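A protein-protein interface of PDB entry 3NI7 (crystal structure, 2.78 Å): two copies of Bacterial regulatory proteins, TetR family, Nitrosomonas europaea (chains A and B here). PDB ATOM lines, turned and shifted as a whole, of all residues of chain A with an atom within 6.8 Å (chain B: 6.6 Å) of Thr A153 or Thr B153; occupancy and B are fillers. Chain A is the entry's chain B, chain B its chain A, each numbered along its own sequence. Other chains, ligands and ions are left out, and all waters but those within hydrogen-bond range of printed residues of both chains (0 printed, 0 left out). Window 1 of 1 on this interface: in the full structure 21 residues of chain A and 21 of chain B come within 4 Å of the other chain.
OG of Ser A150 is in hydrogen-bond range of OG of Ser B126, 3.5 Å away. OG of Ser B126 is in hydrogen-bond range of OG1 of Thr A151. The side-chain carboxylate of Glu A148 sits close to the side-chain carboxylate of Glu B149 (2.6 Å). The side-chain hydroxyl of Ser A150 is in hydrogen-bond range of the side-chain carboxylate of Glu B149, at 2.8 Å. OE2 of Glu A149 is in hydrogen-bond range of OG of Ser B150, 2.7 Å away. OG1 of Thr B151 sits at hydrogen-bond distance from OG of Ser A126, at 3.0 Å.
OG1 of Thr B153 lies within hydrogen-bond range of O of Glu B149, at 2.8 Å. O of Ser B150 sits at hydrogen-bond distance from OG1 of Thr B154, at 2.7 Å. The backbone carbonyl oxygen (O) of Glu A149 lies within hydrogen-bond range of the side-chain hydroxyl (OG1) of Thr A153 (2.8 Å). O of Ser A150 is in hydrogen-bond range of OG1 of Thr A154 (2.6 Å).
OG1 of Thr B154 touches CG1 of Val A125, 3.2 Å away. OG of Ser B150 touches OG of Ser A126, at 3.7 Å. Glu B148 touches Glu A149. Thr B153 touches Ser A150. Thr A153 touches Ser B150 (OG1 to CB, 3.2 Å). Thr A153 touches Thr B153. OG1 of Thr B154 touches CG2 of Thr A153, at 3.5 Å. OG1 of Thr A154 touches CG1 of Val B125, 3.2 Å away. Thr A154 touches Thr B153 (OG1 to CG2, 3.6 Å). CD1 of Leu A157 touches CD1 of Leu B157, at 3.4 Å.
Of the printed residues of chain B, Val A125 touches Thr B154 (3.2 Å). Val A129 touches none of the printed residues of chain B. Thr A153 touches just these residues of chain B: Ser B150, Thr B153 and Thr B154. Of the printed residues of chain B, Leu A157 touches Leu B157. Printed residues of chain A within 4 Å of Ser B126: Ser A150 and Thr A151. Of the printed residues of chain A, Glu B148 touches Glu A149 (3.7 Å). Thr B153 touches just these residues of chain A: Ser A150 (3.2 Å), Thr A153 (3.98 Å) and Thr A154 (3.6 Å). The nearest residue of chain A that does not touch Thr B153 is Leu A157 (5.2 Å). The nearest printed residue of chain A that does not touch Leu B157 is Thr A154 (4.3 Å).
Along chain A the printed residues that touch a printed residue of chain B span positions 125 to 157. Printed residues of chain B that touch a printed residue of chain A: Val B125, Ser B126, Glu B148, Glu B149, Ser B150, Thr B151, Thr B153, Thr B154 and Leu B157.
Glu A148 touches Glu B149, and with the chains exchanged Glu A149 touches Glu B148. Glu A149 touches Ser B150, and with the chains exchanged Ser A150 touches Glu B149. Ser A150 touches Thr B153, and with the chains exchanged Thr A153 touches Ser B150. Thr A153 touches its own counterpart, Thr B153. Positions printed for both chains: 125, 126, 129, 148, 149, 150, 151, 152, 153, 154, 155, 156, 157 and 158.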
ATOM      1  N   VAL A 125      20.414 -22.609  16.177  1.00  0.00           N
ATOM      2  CA  VAL A 125      21.084 -22.390  17.442  1.00  0.00           C
ATOM      3  C   VAL A 125      20.300 -21.414  18.317  1.00  0.00           C
ATOM      4  O   VAL A 125      20.128 -21.680  19.489  1.00  0.00           O
ATOM      5  CB  VAL A 125      22.531 -21.837  17.240  1.00  0.00           C
ATOM      6  CG1 VAL A 125      23.056 -21.226  18.494  1.00  0.00           C
ATOM      7  CG2 VAL A 125      23.492 -22.921  16.704  1.00  0.00           C
ATOM      8  N   SER A 126      19.856 -20.280  17.794  1.00  0.00           N
ATOM      9  CA  SER A 126      19.193 -19.331  18.666  1.00  0.00           C
ATOM     10  C   SER A 126      17.911 -19.903  19.222  1.00  0.00           C
ATOM     11  O   SER A 126      17.663 -19.814  20.427  1.00  0.00           O
ATOM     12  CB  SER A 126      18.920 -18.024  17.989  1.00  0.00           C
ATOM     13  OG  SER A 126      20.114 -17.419  17.587  1.00  0.00           O
ATOM     14  N   VAL A 129      18.817 -22.569  21.877  1.00  0.00           N
ATOM     15  CA  VAL A 129      19.306 -21.948  23.091  1.00  0.00           C
ATOM     16  C   VAL A 129      18.171 -21.260  23.849  1.00  0.00           C
ATOM     17  O   VAL A 129      18.062 -21.357  25.035  1.00  0.00           O
ATOM     18  CB  VAL A 129      20.443 -20.960  22.755  1.00  0.00           C
ATOM     19  CG1 VAL A 129      20.634 -19.956  23.877  1.00  0.00           C
ATOM     20  CG2 VAL A 129      21.746 -21.731  22.468  1.00  0.00           C
ATOM     21  N   LEU A 147      20.809 -16.619  33.714  1.00  0.00           N
ATOM     22  CA  LEU A 147      22.013 -16.907  32.936  1.00  0.00           C
ATOM     23  C   LEU A 147      21.923 -16.110  31.652  1.00  0.00           C
ATOM     24  O   LEU A 147      20.937 -16.219  30.953  1.00  0.00           O
ATOM     25  CB  LEU A 147      22.047 -18.393  32.613  1.00  0.00           C
ATOM     26  CG  LEU A 147      23.313 -18.867  31.970  1.00  0.00           C
ATOM     27  CD1 LEU A 147      24.221 -18.629  32.976  1.00  0.00           C
ATOM     28  CD2 LEU A 147      23.345 -20.312  31.694  1.00  0.00           C
ATOM     29  N   GLU A 148      22.945 -15.322  31.342  1.00  0.00           N
ATOM     30  CA  GLU A 148      22.894 -14.467  30.169  1.00  0.00           C
ATOM     31  C   GLU A 148      22.859 -15.293  28.867  1.00  0.00           C
ATOM     32  O   GLU A 148      23.526 -16.318  28.737  1.00  0.00           O
ATOM     33  CB  GLU A 148      24.005 -13.409  30.161  1.00  0.00           C
ATOM     34  CG  GLU A 148      23.544 -12.068  30.695  1.00  0.00           C
ATOM     35  CD  GLU A 148      22.499 -11.371  29.704  1.00  0.00           C
ATOM     36  OE1 GLU A 148      22.536 -10.125  29.574  1.00  0.00           O
ATOM     37  OE2 GLU A 148      21.633 -12.054  29.034  1.00  0.00           O
ATOM     38  N   GLU A 149      22.019 -14.864  27.934  1.00  0.00           N
ATOM     39  CA  GLU A 149      21.875 -15.566  26.676  1.00  0.00           C
ATOM     40  C   GLU A 149      23.228 -15.923  26.049  1.00  0.00           C
ATOM     41  O   GLU A 149      23.476 -17.070  25.711  1.00  0.00           O
ATOM     42  CB  GLU A 149      21.078 -14.713  25.702  1.00  0.00           C
ATOM     43  CG  GLU A 149      19.554 -14.988  25.606  1.00  0.00           C
ATOM     44  CD  GLU A 149      18.979 -14.406  24.337  1.00  0.00           C
ATOM     45  OE1 GLU A 149      18.368 -13.327  24.397  1.00  0.00           O
ATOM     46  OE2 GLU A 149      19.203 -15.000  23.275  1.00  0.00           O
ATOM     47  N   SER A 150      24.108 -14.944  25.915  1.00  0.00           N
ATOM     48  CA  SER A 150      25.437 -15.196  25.330  1.00  0.00           C
ATOM     49  C   SER A 150      26.246 -16.241  26.051  1.00  0.00           C
ATOM     50  O   SER A 150      26.879 -17.081  25.394  1.00  0.00           O
ATOM     51  CB  SER A 150      26.277 -13.932  25.247  1.00  0.00           C
ATOM     52  OG  SER A 150      26.041 -13.079  26.334  1.00  0.00           O
ATOM     53  N   THR A 151      26.214 -16.190  27.385  1.00  0.00           N
ATOM     54  CA  THR A 151      26.961 -17.100  28.178  1.00  0.00           C
ATOM     55  C   THR A 151      26.546 -18.492  27.863  1.00  0.00           C
ATOM     56  O   THR A 151      27.324 -19.339  27.451  1.00  0.00           O
ATOM     57  CB  THR A 151      26.712 -16.859  29.618  1.00  0.00           C
ATOM     58  OG1 THR A 151      27.088 -15.505  29.924  1.00  0.00           O
ATOM     59  CG2 THR A 151      27.562 -17.841  30.438  1.00  0.00           C
ATOM     60  N   LEU A 152      25.266 -18.720  28.015  1.00  0.00           N
ATOM     61  CA  LEU A 152      24.691 -20.016  27.684  1.00  0.00           C
ATOM     62  C   LEU A 152      24.953 -20.413  26.247  1.00  0.00           C
ATOM     63  O   LEU A 152      25.200 -21.576  25.949  1.00  0.00           O
ATOM     64  CB  LEU A 152      23.221 -19.990  27.984  1.00  0.00           C
ATOM     65  CG  LEU A 152      22.537 -21.309  27.677  1.00  0.00           C
ATOM     66  CD1 LEU A 152      23.312 -22.530  28.146  1.00  0.00           C
ATOM     67  CD2 LEU A 152      21.118 -21.260  28.265  1.00  0.00           C
ATOM     68  N   THR A 153      24.910 -19.447  25.356  1.00  0.00           N
ATOM     69  CA  THR A 153      25.157 -19.771  23.945  1.00  0.00           C
ATOM     70  C   THR A 153      26.593 -20.229  23.847  1.00  0.00           C
ATOM     71  O   THR A 153      26.900 -21.295  23.278  1.00  0.00           O
ATOM     72  CB  THR A 153      24.966 -18.567  22.983  1.00  0.00           C
ATOM     73  OG1 THR A 153      23.634 -18.110  23.073  1.00  0.00           O
ATOM     74  CG2 THR A 153      25.257 -18.964  21.609  1.00  0.00           C
ATOM     75  N   THR A 154      27.467 -19.407  24.417  1.00  0.00           N
ATOM     76  CA  THR A 154      28.867 -19.665  24.309  1.00  0.00           C
ATOM     77  C   THR A 154      29.134 -21.035  24.853  1.00  0.00           C
ATOM     78  O   THR A 154      29.930 -21.782  24.283  1.00  0.00           O
ATOM     79  CB  THR A 154      29.648 -18.623  25.039  1.00  0.00           C
ATOM     80  OG1 THR A 154      29.329 -17.355  24.458  1.00  0.00           O
ATOM     81  CG2 THR A 154      31.125 -18.878  24.897  1.00  0.00           C
ATOM     82  N   ILE A 155      28.427 -21.390  25.919  1.00  0.00           N
ATOM     83  CA  ILE A 155      28.667 -22.672  26.546  1.00  0.00           C
ATOM     84  C   ILE A 155      28.120 -23.782  25.697  1.00  0.00           C
ATOM     85  O   ILE A 155      28.723 -24.812  25.498  1.00  0.00           O
ATOM     86  CB  ILE A 155      28.090 -22.774  27.963  1.00  0.00           C
ATOM     87  CG1 ILE A 155      28.839 -21.855  28.946  1.00  0.00           C
ATOM     88  CG2 ILE A 155      28.242 -24.219  28.484  1.00  0.00           C
ATOM     89  CD1 ILE A 155      28.070 -21.533  30.239  1.00  0.00           C
ATOM     90  N   TYR A 156      26.951 -23.580  25.175  1.00  0.00           N
ATOM     91  CA  TYR A 156      26.359 -24.644  24.402  1.00  0.00           C
ATOM     92  C   TYR A 156      27.244 -24.896  23.163  1.00  0.00           C
ATOM     93  O   TYR A 156      27.657 -26.015  22.882  1.00  0.00           O
ATOM     94  CB  TYR A 156      24.927 -24.280  24.102  1.00  0.00           C
ATOM     95  CG  TYR A 156      24.250 -25.092  23.046  1.00  0.00           C
ATOM     96  CD1 TYR A 156      23.674 -26.332  23.325  1.00  0.00           C
ATOM     97  CD2 TYR A 156      24.103 -24.566  21.760  1.00  0.00           C
ATOM     98  CE1 TYR A 156      22.995 -27.052  22.326  1.00  0.00           C
ATOM     99  CE2 TYR A 156      23.463 -25.261  20.741  1.00  0.00           C
ATOM    100  CZ  TYR A 156      22.909 -26.501  21.016  1.00  0.00           C
ATOM    101  OH  TYR A 156      22.296 -27.155  19.960  1.00  0.00           O
ATOM    102  N   LEU A 157      27.621 -23.836  22.489  1.00  0.00           N
ATOM    103  CA  LEU A 157      28.542 -23.977  21.388  1.00  0.00           C
ATOM    104  C   LEU A 157      29.800 -24.739  21.734  1.00  0.00           C
ATOM    105  O   LEU A 157      30.128 -25.709  21.077  1.00  0.00           O
ATOM    106  CB  LEU A 157      28.908 -22.607  20.827  1.00  0.00           C
ATOM    107  CG  LEU A 157      27.792 -22.047  19.900  1.00  0.00           C
ATOM    108  CD1 LEU A 157      28.168 -20.781  19.131  1.00  0.00           C
ATOM    109  CD2 LEU A 157      27.402 -23.068  18.882  1.00  0.00           C
ATOM    110  N   MET A 158      30.489 -24.306  22.789  1.00  0.00           N
ATOM    111  CA  MET A 158      31.781 -24.883  23.138  1.00  0.00           C
ATOM    112  C   MET A 158      31.666 -26.315  23.546  1.00  0.00           C
ATOM    113  O   MET A 158      32.516 -27.130  23.243  1.00  0.00           O
ATOM    114  CB  MET A 158      32.381 -24.146  24.270  1.00  0.00           C
ATOM    115  CG  MET A 158      33.383 -23.098  23.932  1.00  0.00           C
ATOM    116  SD  MET A 158      34.024 -22.471  25.749  1.00  0.00           S
ATOM    117  CE  MET A 158      35.758 -21.632  25.261  1.00  0.00           C
ATOM    118  N   THR A 159      30.609 -26.621  24.265  1.00  0.00           N
ATOM    119  CA  THR A 159      30.398 -27.992  24.707  1.00  0.00           C
ATOM    120  C   THR A 159      30.247 -28.852  23.485  1.00  0.00           C
ATOM    121  O   THR A 159      30.862 -29.908  23.350  1.00  0.00           O
ATOM    122  CB  THR A 159      29.153 -28.146  25.556  1.00  0.00           C
ATOM    123  OG1 THR A 159      29.211 -27.204  26.627  1.00  0.00           O
ATOM    124  CG2 THR A 159      29.063 -29.567  26.102  1.00  0.00           C
ATOM    125  N   VAL B 125      33.908 -13.401  26.164  1.00  0.00           N
ATOM    126  CA  VAL B 125      32.978 -13.403  25.056  1.00  0.00           C
ATOM    127  C   VAL B 125      31.714 -12.605  25.376  1.00  0.00           C
ATOM    128  O   VAL B 125      31.330 -11.741  24.602  1.00  0.00           O
ATOM    129  CB  VAL B 125      32.604 -14.842  24.682  1.00  0.00           C
ATOM    130  CG1 VAL B 125      31.332 -14.886  23.888  1.00  0.00           C
ATOM    131  CG2 VAL B 125      33.736 -15.498  23.907  1.00  0.00           C
ATOM    132  N   SER B 126      31.069 -12.887  26.506  1.00  0.00           N
ATOM    133  CA  SER B 126      29.808 -12.238  26.831  1.00  0.00           C
ATOM    134  C   SER B 126      29.989 -10.744  26.925  1.00  0.00           C
ATOM    135  O   SER B 126      29.284  -9.998  26.275  1.00  0.00           O
ATOM    136  CB  SER B 126      29.208 -12.757  28.127  1.00  0.00           C
ATOM    137  OG  SER B 126      28.917 -14.127  28.005  1.00  0.00           O
ATOM    138  N   VAL B 129      30.539  -9.333  23.417  1.00  0.00           N
ATOM    139  CA  VAL B 129      29.321  -9.340  22.675  1.00  0.00           C
ATOM    140  C   VAL B 129      28.380  -8.285  23.187  1.00  0.00           C
ATOM    141  O   VAL B 129      27.683  -7.637  22.396  1.00  0.00           O
ATOM    142  CB  VAL B 129      28.665 -10.741  22.720  1.00  0.00           C
ATOM    143  CG1 VAL B 129      27.121 -10.694  22.446  1.00  0.00           C
ATOM    144  CG2 VAL B 129      29.395 -11.667  21.717  1.00  0.00           C
ATOM    145  N   GLU B 148      19.122 -10.578  18.401  1.00  0.00           N
ATOM    146  CA  GLU B 148      19.041 -11.361  19.600  1.00  0.00           C
ATOM    147  C   GLU B 148      20.515 -11.677  20.012  1.00  0.00           C
ATOM    148  O   GLU B 148      21.412 -11.926  19.148  1.00  0.00           O
ATOM    149  CB  GLU B 148      18.193 -12.624  19.433  1.00  0.00           C
ATOM    150  CG  GLU B 148      16.725 -12.344  19.287  1.00  0.00           C
ATOM    151  CD  GLU B 148      16.136 -11.525  20.432  1.00  0.00           C
ATOM    152  OE1 GLU B 148      16.375 -11.836  21.656  1.00  0.00           O
ATOM    153  OE2 GLU B 148      15.394 -10.564  20.093  1.00  0.00           O
ATOM    154  N   GLU B 149      20.727 -11.614  21.339  1.00  0.00           N
ATOM    155  CA  GLU B 149      22.010 -11.867  21.940  1.00  0.00           C
ATOM    156  C   GLU B 149      22.638 -13.150  21.426  1.00  0.00           C
ATOM    157  O   GLU B 149      23.815 -13.154  21.104  1.00  0.00           O
ATOM    158  CB  GLU B 149      21.887 -11.970  23.467  1.00  0.00           C
ATOM    159  CG  GLU B 149      22.213 -10.694  24.310  1.00  0.00           C
ATOM    160  CD  GLU B 149      22.559 -11.033  25.771  1.00  0.00           C
ATOM    161  OE1 GLU B 149      21.704 -10.861  26.692  1.00  0.00           O
ATOM    162  OE2 GLU B 149      23.700 -11.499  26.008  1.00  0.00           O
ATOM    163  N   SER B 150      21.886 -14.246  21.369  1.00  0.00           N
ATOM    164  CA  SER B 150      22.447 -15.513  20.837  1.00  0.00           C
ATOM    165  C   SER B 150      22.805 -15.474  19.350  1.00  0.00           C
ATOM    166  O   SER B 150      23.756 -16.108  18.904  1.00  0.00           O
ATOM    167  CB  SER B 150      21.532 -16.689  21.095  1.00  0.00           C
ATOM    168  OG  SER B 150      20.202 -16.258  21.061  1.00  0.00           O
ATOM    169  N   THR B 151      22.048 -14.729  18.576  1.00  0.00           N
ATOM    170  CA  THR B 151      22.292 -14.725  17.157  1.00  0.00           C
ATOM    171  C   THR B 151      23.624 -14.065  17.005  1.00  0.00           C
ATOM    172  O   THR B 151      24.609 -14.647  16.497  1.00  0.00           O
ATOM    173  CB  THR B 151      21.215 -13.947  16.402  1.00  0.00           C
ATOM    174  OG1 THR B 151      19.965 -14.632  16.532  1.00  0.00           O
ATOM    175  CG2 THR B 151      21.570 -13.811  14.965  1.00  0.00           C
ATOM    176  N   LEU B 152      23.671 -12.841  17.488  1.00  0.00           N
ATOM    177  CA  LEU B 152      24.930 -12.104  17.436  1.00  0.00           C
ATOM    178  C   LEU B 152      26.095 -12.883  18.078  1.00  0.00           C
ATOM    179  O   LEU B 152      27.203 -12.830  17.595  1.00  0.00           O
ATOM    180  CB  LEU B 152      24.771 -10.805  18.176  1.00  0.00           C
ATOM    181  CG  LEU B 152      26.007  -9.957  18.208  1.00  0.00           C
ATOM    182  CD1 LEU B 152      26.617  -9.849  16.841  1.00  0.00           C
ATOM    183  CD2 LEU B 152      25.544  -8.634  18.773  1.00  0.00           C
ATOM    184  N   THR B 153      25.844 -13.622  19.132  1.00  0.00           N
ATOM    185  CA  THR B 153      26.937 -14.388  19.700  1.00  0.00           C
ATOM    186  C   THR B 153      27.342 -15.450  18.722  1.00  0.00           C
ATOM    187  O   THR B 153      28.536 -15.626  18.444  1.00  0.00           O
ATOM    188  CB  THR B 153      26.598 -15.084  21.059  1.00  0.00           C
ATOM    189  OG1 THR B 153      26.318 -14.085  22.046  1.00  0.00           O
ATOM    190  CG2 THR B 153      27.776 -15.884  21.532  1.00  0.00           C
ATOM    191  N   THR B 154      26.345 -16.166  18.209  1.00  0.00           N
ATOM    192  CA  THR B 154      26.629 -17.290  17.361  1.00  0.00           C
ATOM    193  C   THR B 154      27.363 -16.789  16.163  1.00  0.00           C
ATOM    194  O   THR B 154      28.230 -17.458  15.644  1.00  0.00           O
ATOM    195  CB  THR B 154      25.382 -17.981  16.955  1.00  0.00           C
ATOM    196  OG1 THR B 154      24.773 -18.535  18.141  1.00  0.00           O
ATOM    197  CG2 THR B 154      25.698 -19.095  15.951  1.00  0.00           C
ATOM    198  N   ILE B 155      27.046 -15.576  15.743  1.00  0.00           N
ATOM    199  CA  ILE B 155      27.722 -15.011  14.576  1.00  0.00           C
ATOM    200  C   ILE B 155      29.140 -14.616  14.905  1.00  0.00           C
ATOM    201  O   ILE B 155      30.078 -14.831  14.121  1.00  0.00           O
ATOM    202  CB  ILE B 155      26.962 -13.799  13.949  1.00  0.00           C
ATOM    203  CG1 ILE B 155      25.618 -14.261  13.308  1.00  0.00           C
ATOM    204  CG2 ILE B 155      27.811 -13.155  12.866  1.00  0.00           C
ATOM    205  CD1 ILE B 155      24.534 -13.145  13.119  1.00  0.00           C
ATOM    206  N   TYR B 156      29.313 -14.023  16.068  1.00  0.00           N
ATOM    207  CA  TYR B 156      30.647 -13.528  16.415  1.00  0.00           C
ATOM    208  C   TYR B 156      31.592 -14.702  16.622  1.00  0.00           C
ATOM    209  O   TYR B 156      32.644 -14.778  16.034  1.00  0.00           O
ATOM    210  CB  TYR B 156      30.549 -12.594  17.554  1.00  0.00           C
ATOM    211  CG  TYR B 156      31.805 -12.276  18.243  1.00  0.00           C
ATOM    212  CD1 TYR B 156      32.637 -11.232  17.835  1.00  0.00           C
ATOM    213  CD2 TYR B 156      32.130 -12.961  19.410  1.00  0.00           C
ATOM    214  CE1 TYR B 156      33.817 -10.927  18.558  1.00  0.00           C
ATOM    215  CE2 TYR B 156      33.284 -12.682  20.119  1.00  0.00           C
ATOM    216  CZ  TYR B 156      34.110 -11.675  19.702  1.00  0.00           C
ATOM    217  OH  TYR B 156      35.199 -11.482  20.522  1.00  0.00           O
ATOM    218  N   LEU B 157      31.127 -15.703  17.313  1.00  0.00           N
ATOM    219  CA  LEU B 157      31.865 -16.946  17.353  1.00  0.00           C
ATOM    220  C   LEU B 157      32.217 -17.508  15.982  1.00  0.00           C
ATOM    221  O   LEU B 157      33.369 -17.776  15.699  1.00  0.00           O
ATOM    222  CB  LEU B 157      31.073 -17.995  18.133  1.00  0.00           C
ATOM    223  CG  LEU B 157      31.137 -17.716  19.629  1.00  0.00           C
ATOM    224  CD1 LEU B 157      30.608 -18.860  20.418  1.00  0.00           C
ATOM    225  CD2 LEU B 157      32.525 -17.509  19.984  1.00  0.00           C
ATOM    226  N   MET B 158      31.220 -17.713  15.133  1.00  0.00           N
ATOM    227  CA  MET B 158      31.468 -18.405  13.862  1.00  0.00           C
ATOM    228  C   MET B 158      32.429 -17.642  12.982  1.00  0.00           C
ATOM    229  O   MET B 158      33.384 -18.206  12.432  1.00  0.00           O
ATOM    230  CB  MET B 158      30.206 -18.568  13.087  1.00  0.00           C
ATOM    231  CG  MET B 158      29.537 -19.900  13.193  1.00  0.00           C
ATOM    232  SD  MET B 158      28.092 -19.797  11.749  1.00  0.00           S
ATOM    233  CE  MET B 158      27.497 -21.705  11.787  1.00  0.00           C
